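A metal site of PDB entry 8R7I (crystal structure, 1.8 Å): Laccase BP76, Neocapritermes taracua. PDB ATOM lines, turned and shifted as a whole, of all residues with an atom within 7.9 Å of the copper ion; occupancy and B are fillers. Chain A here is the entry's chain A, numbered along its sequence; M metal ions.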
ATOM      1  N   VAL A 272       3.552 -35.328  10.705  1.00  0.00           N
ATOM      2  CA  VAL A 272       3.674 -34.197  11.646  1.00  0.00           C
ATOM      3  C   VAL A 272       3.218 -34.548  13.079  1.00  0.00           C
ATOM      4  O   VAL A 272       3.106 -33.643  13.902  1.00  0.00           O
ATOM      5  CB  VAL A 272       2.873 -32.982  11.104  1.00  0.00           C
ATOM      6  CG1 VAL A 272       3.442 -32.467   9.797  1.00  0.00           C
ATOM      7  CG2 VAL A 272       1.389 -33.302  10.943  1.00  0.00           C
ATOM      8  N   PHE A 414      11.544 -20.671   9.555  1.00  0.00           N
ATOM      9  CA  PHE A 414      10.951 -21.743   8.764  1.00  0.00           C
ATOM     10  C   PHE A 414       9.433 -21.575   8.761  1.00  0.00           C
ATOM     11  O   PHE A 414       8.826 -21.072   9.745  1.00  0.00           O
ATOM     12  CB  PHE A 414      11.370 -23.132   9.278  1.00  0.00           C
ATOM     13  CG  PHE A 414      11.001 -23.436  10.697  1.00  0.00           C
ATOM     14  CD1 PHE A 414       9.745 -23.878  11.036  1.00  0.00           C
ATOM     15  CD2 PHE A 414      11.939 -23.279  11.729  1.00  0.00           C
ATOM     16  CE1 PHE A 414       9.409 -24.151  12.348  1.00  0.00           C
ATOM     17  CE2 PHE A 414      11.615 -23.547  13.039  1.00  0.00           C
ATOM     18  CZ  PHE A 414      10.329 -23.966  13.354  1.00  0.00           C
ATOM     19  N   GLY A 415       8.807 -21.989   7.660  1.00  0.00           N
ATOM     20  CA  GLY A 415       7.359 -22.003   7.609  1.00  0.00           C
ATOM     21  C   GLY A 415       6.855 -22.334   6.210  1.00  0.00           C
ATOM     22  O   GLY A 415       7.492 -23.105   5.488  1.00  0.00           O
ATOM     23  N   PHE A 416       5.706 -21.744   5.872  1.00  0.00           N
ATOM     24  CA  PHE A 416       4.961 -22.048   4.649  1.00  0.00           C
ATOM     25  C   PHE A 416       4.607 -20.777   3.882  1.00  0.00           C
ATOM     26  O   PHE A 416       4.310 -19.721   4.513  1.00  0.00           O
ATOM     27  CB  PHE A 416       3.675 -22.767   4.985  1.00  0.00           C
ATOM     28  CG  PHE A 416       3.881 -24.036   5.757  1.00  0.00           C
ATOM     29  CD1 PHE A 416       4.489 -25.137   5.150  1.00  0.00           C
ATOM     30  CD2 PHE A 416       3.478 -24.142   7.072  1.00  0.00           C
ATOM     31  CE1 PHE A 416       4.692 -26.318   5.858  1.00  0.00           C
ATOM     32  CE2 PHE A 416       3.685 -25.328   7.789  1.00  0.00           C
ATOM     33  CZ  PHE A 416       4.288 -26.400   7.174  1.00  0.00           C
ATOM     34  N   PHE A 435       1.538 -28.727  -1.615  1.00  0.00           N
ATOM     35  CA  PHE A 435       0.907 -29.854  -0.949  1.00  0.00           C
ATOM     36  C   PHE A 435      -0.357 -29.349  -0.265  1.00  0.00           C
ATOM     37  O   PHE A 435      -0.445 -28.166   0.075  1.00  0.00           O
ATOM     38  CB  PHE A 435       1.903 -30.652  -0.061  1.00  0.00           C
ATOM     39  CG  PHE A 435       2.237 -30.083   1.289  1.00  0.00           C
ATOM     40  CD1 PHE A 435       2.986 -28.918   1.414  1.00  0.00           C
ATOM     41  CD2 PHE A 435       1.953 -30.818   2.437  1.00  0.00           C
ATOM     42  CE1 PHE A 435       3.356 -28.454   2.674  1.00  0.00           C
ATOM     43  CE2 PHE A 435       2.331 -30.357   3.692  1.00  0.00           C
ATOM     44  CZ  PHE A 435       3.025 -29.167   3.793  1.00  0.00           C
ATOM     45  N   SER A 445       6.938 -25.154   1.340  1.00  0.00           N
ATOM     46  CA  SER A 445       7.711 -24.909   2.546  1.00  0.00           C
ATOM     47  C   SER A 445       8.850 -23.923   2.237  1.00  0.00           C
ATOM     48  O   SER A 445       9.382 -23.941   1.128  1.00  0.00           O
ATOM     49  CB  SER A 445       8.224 -26.197   3.200  1.00  0.00           C
ATOM     50  OG  SER A 445       7.125 -27.010   3.577  1.00  0.00           O
ATOM     51  N   ASP A 512       9.599 -20.796  14.271  1.00  0.00           N
ATOM     52  CA  ASP A 512       8.305 -21.110  13.674  1.00  0.00           C
ATOM     53  C   ASP A 512       7.598 -19.798  13.293  1.00  0.00           C
ATOM     54  O   ASP A 512       6.735 -19.332  14.060  1.00  0.00           O
ATOM     55  CB  ASP A 512       7.481 -21.933  14.666  1.00  0.00           C
ATOM     56  CG  ASP A 512       6.188 -22.523  14.137  1.00  0.00           C
ATOM     57  OD1 ASP A 512       6.141 -22.867  12.928  1.00  0.00           O
ATOM     58  OD2 ASP A 512       5.291 -22.720  14.953  1.00  0.00           O
ATOM     59  N   LEU A 519       1.949 -27.327  15.260  1.00  0.00           N
ATOM     60  CA  LEU A 519       3.122 -28.040  14.729  1.00  0.00           C
ATOM     61  C   LEU A 519       4.386 -27.759  15.537  1.00  0.00           C
ATOM     62  O   LEU A 519       4.783 -26.577  15.751  1.00  0.00           O
ATOM     63  CB  LEU A 519       3.341 -27.684  13.256  1.00  0.00           C
ATOM     64  CG  LEU A 519       2.284 -28.175  12.280  1.00  0.00           C
ATOM     65  CD1 LEU A 519       2.426 -27.497  10.927  1.00  0.00           C
ATOM     66  CD2 LEU A 519       2.372 -29.680  12.153  1.00  0.00           C
ATOM     67  N   HIS A 520       5.108 -28.834  15.883  1.00  0.00           N
ATOM     68  CA  HIS A 520       6.418 -28.816  16.543  1.00  0.00           C
ATOM     69  C   HIS A 520       7.441 -29.391  15.547  1.00  0.00           C
ATOM     70  O   HIS A 520       7.724 -30.595  15.566  1.00  0.00           O
ATOM     71  CB  HIS A 520       6.370 -29.641  17.845  1.00  0.00           C
ATOM     72  CG  HIS A 520       5.680 -28.955  18.954  1.00  0.00           C
ATOM     73  ND1 HIS A 520       4.361 -28.603  18.883  1.00  0.00           N
ATOM     74  CD2 HIS A 520       6.137 -28.533  20.179  1.00  0.00           C
ATOM     75  CE1 HIS A 520       4.010 -28.016  20.036  1.00  0.00           C
ATOM     76  NE2 HIS A 520       5.065 -27.955  20.840  1.00  0.00           N
ATOM     77  N   HIS A 521       7.960 -28.536  14.667  1.00  0.00           N
ATOM     78  CA  HIS A 521       8.789 -28.965  13.527  1.00  0.00           C
ATOM     79  C   HIS A 521      10.123 -29.449  14.064  1.00  0.00           C
ATOM     80  O   HIS A 521      10.857 -28.679  14.743  1.00  0.00           O
ATOM     81  CB  HIS A 521       9.014 -27.802  12.553  1.00  0.00           C
ATOM     82  CG  HIS A 521       7.789 -27.262  11.913  1.00  0.00           C
ATOM     83  ND1 HIS A 521       7.396 -27.580  10.639  1.00  0.00           N
ATOM     84  CD2 HIS A 521       6.853 -26.346  12.405  1.00  0.00           C
ATOM     85  CE1 HIS A 521       6.311 -26.859  10.337  1.00  0.00           C
ATOM     86  NE2 HIS A 521       5.969 -26.101  11.390  1.00  0.00           N
ATOM     87  N   PRO A 522      10.512 -30.729  13.845  1.00  0.00           N
ATOM     88  CA  PRO A 522      11.779 -31.229  14.367  1.00  0.00           C
ATOM     89  C   PRO A 522      12.927 -31.092  13.390  1.00  0.00           C
ATOM     90  O   PRO A 522      13.021 -31.821  12.422  1.00  0.00           O
ATOM     91  CB  PRO A 522      11.455 -32.696  14.675  1.00  0.00           C
ATOM     92  CG  PRO A 522      10.407 -33.069  13.634  1.00  0.00           C
ATOM     93  CD  PRO A 522       9.667 -31.789  13.264  1.00  0.00           C
ATOM     94  N   PHE A 523      13.826 -30.149  13.641  1.00  0.00           N
ATOM     95  CA  PHE A 523      14.957 -29.880  12.747  1.00  0.00           C
ATOM     96  C   PHE A 523      16.135 -30.778  13.078  1.00  0.00           C
ATOM     97  O   PHE A 523      16.504 -30.938  14.237  1.00  0.00           O
ATOM     98  CB  PHE A 523      15.328 -28.388  12.813  1.00  0.00           C
ATOM     99  CG  PHE A 523      14.475 -27.599  11.859  1.00  0.00           C
ATOM    100  CD1 PHE A 523      13.195 -27.212  12.242  1.00  0.00           C
ATOM    101  CD2 PHE A 523      14.906 -27.360  10.561  1.00  0.00           C
ATOM    102  CE1 PHE A 523      12.376 -26.536  11.338  1.00  0.00           C
ATOM    103  CE2 PHE A 523      14.066 -26.731   9.655  1.00  0.00           C
ATOM    104  CZ  PHE A 523      12.792 -26.328  10.055  1.00  0.00           C
ATOM    105  N   HIS A 591      17.315 -29.844   8.049  1.00  0.00           N
ATOM    106  CA  HIS A 591      15.947 -29.809   7.499  1.00  0.00           C
ATOM    107  C   HIS A 591      14.924 -30.267   8.528  1.00  0.00           C
ATOM    108  O   HIS A 591      15.265 -30.960   9.523  1.00  0.00           O
ATOM    109  CB  HIS A 591      15.878 -30.644   6.227  1.00  0.00           C
ATOM    110  CG  HIS A 591      16.104 -32.080   6.468  1.00  0.00           C
ATOM    111  ND1 HIS A 591      15.076 -32.914   6.911  1.00  0.00           N
ATOM    112  CD2 HIS A 591      17.212 -32.863   6.336  1.00  0.00           C
ATOM    113  CE1 HIS A 591      15.571 -34.159   7.033  1.00  0.00           C
ATOM    114  NE2 HIS A 591      16.837 -34.137   6.653  1.00  0.00           N
ATOM    115  N   CYS A 592      13.663 -29.880   8.270  1.00  0.00           N
ATOM    116  CA  CYS A 592      12.565 -30.382   9.072  1.00  0.00           C
ATOM    117  C   CYS A 592      12.470 -31.887   8.797  1.00  0.00           C
ATOM    118  O   CYS A 592      12.528 -32.270   7.643  1.00  0.00           O
ATOM    119  CB  CYS A 592      11.269 -29.681   8.768  1.00  0.00           C
ATOM    120  SG  CYS A 592       9.961 -30.380   9.767  1.00  0.00           S
ATOM    121  N   HIS A 593      12.379 -32.712   9.854  1.00  0.00           N
ATOM    122  CA  HIS A 593      12.357 -34.166   9.680  1.00  0.00           C
ATOM    123  C   HIS A 593      10.954 -34.654   9.284  1.00  0.00           C
ATOM    124  O   HIS A 593      10.820 -35.809   8.815  1.00  0.00           O
ATOM    125  CB  HIS A 593      12.897 -34.886  10.946  1.00  0.00           C
ATOM    126  CG  HIS A 593      13.509 -36.218  10.558  1.00  0.00           C
ATOM    127  ND1 HIS A 593      12.752 -37.373  10.513  1.00  0.00           N
ATOM    128  CD2 HIS A 593      14.758 -36.549  10.168  1.00  0.00           C
ATOM    129  CE1 HIS A 593      13.515 -38.366  10.117  1.00  0.00           C
ATOM    130  NE2 HIS A 593      14.766 -37.913   9.942  1.00  0.00           N
ATOM    131  N   PHE A 594       9.900 -33.815   9.444  1.00  0.00           N
ATOM    132  CA  PHE A 594       8.572 -34.167   8.939  1.00  0.00           C
ATOM    133  C   PHE A 594       8.708 -34.340   7.411  1.00  0.00           C
ATOM    134  O   PHE A 594       9.093 -33.410   6.685  1.00  0.00           O
ATOM    135  CB  PHE A 594       7.539 -33.090   9.289  1.00  0.00           C
ATOM    136  CG  PHE A 594       7.205 -32.929  10.752  1.00  0.00           C
ATOM    137  CD1 PHE A 594       7.342 -33.958  11.671  1.00  0.00           C
ATOM    138  CD2 PHE A 594       6.655 -31.717  11.198  1.00  0.00           C
ATOM    139  CE1 PHE A 594       6.948 -33.810  12.987  1.00  0.00           C
ATOM    140  CE2 PHE A 594       6.273 -31.563  12.511  1.00  0.00           C
ATOM    141  CZ  PHE A 594       6.425 -32.612  13.426  1.00  0.00           C
ATOM    142  N   MET A 595       8.453 -35.572   6.921  1.00  0.00           N
ATOM    143  CA  MET A 595       8.863 -35.993   5.573  1.00  0.00           C
ATOM    144  C   MET A 595       8.234 -35.109   4.473  1.00  0.00           C
ATOM    145  O   MET A 595       8.895 -34.801   3.467  1.00  0.00           O
ATOM    146  CB  MET A 595       8.460 -37.454   5.357  1.00  0.00           C
ATOM    147  CG  MET A 595       8.991 -38.064   4.067  1.00  0.00           C
ATOM    148  SD  MET A 595       8.367 -39.776   3.908  1.00  0.00           S
ATOM    149  CE  MET A 595       6.593 -39.504   3.791  1.00  0.00           C
ATOM    150  N   TYR A 596       6.968 -34.691   4.639  1.00  0.00           N
ATOM    151  CA  TYR A 596       6.265 -33.925   3.621  1.00  0.00           C
ATOM    152  C   TYR A 596       6.734 -32.446   3.650  1.00  0.00           C
ATOM    153  O   TYR A 596       6.517 -31.737   2.681  1.00  0.00           O
ATOM    154  CB  TYR A 596       4.745 -34.065   3.779  1.00  0.00           C
ATOM    155  CG  TYR A 596       4.234 -35.427   3.407  1.00  0.00           C
ATOM    156  CD1 TYR A 596       4.061 -35.813   2.089  1.00  0.00           C
ATOM    157  CD2 TYR A 596       3.973 -36.372   4.396  1.00  0.00           C
ATOM    158  CE1 TYR A 596       3.583 -37.075   1.763  1.00  0.00           C
ATOM    159  CE2 TYR A 596       3.511 -37.646   4.082  1.00  0.00           C
ATOM    160  CZ  TYR A 596       3.343 -38.011   2.759  1.00  0.00           C
ATOM    161  OH  TYR A 596       2.829 -39.273   2.474  1.00  0.00           O
ATOM    162  N   HIS A 597       7.385 -32.022   4.745  1.00  0.00           N
ATOM    163  CA  HIS A 597       7.956 -30.672   4.822  1.00  0.00           C
ATOM    164  C   HIS A 597       9.322 -30.666   4.117  1.00  0.00           C
ATOM    165  O   HIS A 597       9.606 -29.757   3.327  1.00  0.00           O
ATOM    166  CB  HIS A 597       8.017 -30.196   6.281  1.00  0.00           C
ATOM    167  CG  HIS A 597       6.678 -30.059   6.913  1.00  0.00           C
ATOM    168  ND1 HIS A 597       6.551 -29.594   8.184  1.00  0.00           N
ATOM    169  CD2 HIS A 597       5.425 -30.300   6.453  1.00  0.00           C
ATOM    170  CE1 HIS A 597       5.253 -29.580   8.489  1.00  0.00           C
ATOM    171  NE2 HIS A 597       4.537 -29.989   7.441  1.00  0.00           N
ATOM    172  N   LEU A 598      10.175 -31.668   4.382  1.00  0.00           N
ATOM    173  CA  LEU A 598      11.397 -31.854   3.597  1.00  0.00           C
ATOM    174  C   LEU A 598      11.032 -31.901   2.109  1.00  0.00           C
ATOM    175  O   LEU A 598      11.700 -31.275   1.279  1.00  0.00           O
ATOM    176  CB  LEU A 598      12.124 -33.121   4.039  1.00  0.00           C
ATOM    177  CG  LEU A 598      13.282 -33.554   3.161  1.00  0.00           C
ATOM    178  CD1 LEU A 598      14.389 -32.524   3.185  1.00  0.00           C
ATOM    179  CD2 LEU A 598      13.815 -34.921   3.601  1.00  0.00           C
ATOM    180  N   THR A 600       8.792 -30.565   0.434  1.00  0.00           N
ATOM    181  CA  THR A 600       8.312 -29.297  -0.114  1.00  0.00           C
ATOM    182  C   THR A 600       9.250 -28.147   0.257  1.00  0.00           C
ATOM    183  O   THR A 600       8.832 -26.984   0.193  1.00  0.00           O
ATOM    184  CB  THR A 600       6.859 -29.039   0.281  1.00  0.00           C
ATOM    185  OG1 THR A 600       6.740 -29.086   1.705  1.00  0.00           O
ATOM    186  CG2 THR A 600       5.922 -30.042  -0.365  1.00  0.00           C
ATOM    187  N   MET A 602      11.603 -27.519   3.056  1.00  0.00           N
ATOM    188  CA  MET A 602      11.917 -27.020   4.404  1.00  0.00           C
ATOM    189  C   MET A 602      13.327 -27.495   4.817  1.00  0.00           C
ATOM    190  O   MET A 602      13.489 -28.313   5.732  1.00  0.00           O
ATOM    191  CB  MET A 602      10.863 -27.415   5.441  1.00  0.00           C
ATOM    192  CG  MET A 602      10.847 -26.445   6.649  1.00  0.00           C
ATOM    193  SD  MET A 602       9.567 -26.739   7.857  1.00  0.00           S
ATOM    194  CE  MET A 602       8.126 -26.118   7.003  1.00  0.00           C
HETATM  195 CU    CU M   1       8.174 -29.071   9.434  1.00  0.00          CU
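ND1 of His 521 lies close to SD of Met 602.
The backbone carbonyl oxygen of His 597 sits at hydrogen-bond distance from the backbone NH of Met 602 (3.0 Å).
The side-chain hydroxyl of Thr 600 sits at hydrogen-bond distance from the backbone carbonyl oxygen of His 597, 3.4 Å away.
The backbone carbonyl oxygen (O) of Met 602 is in hydrogen-bond range of the backbone NH (N) of Cys 592 (3.0 Å).
SG of Cys 592 sits close to N of Phe 594, 3.5 Å away.
Phe 594 touches the copper ion (CD2 to CU, 3.5 Å).
Met 602 touches the copper ion (SD to CU, 3.1 Å).
Five residues have an atom within 4 Å of the copper ion: His 521, Cys 592, Phe 594, His 597 and Met 602.
The nearest printed residue that does not touch the copper ion is Pro 522 (4.9 Å).
The copper ion is bound by a ring nitrogen (ND1) of His 521 (2.1 Å), a ring nitrogen (ND1) of His 597 (2.1 Å) and the side-chain sulfur (SG) of Cys 592 (2.2 Å).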
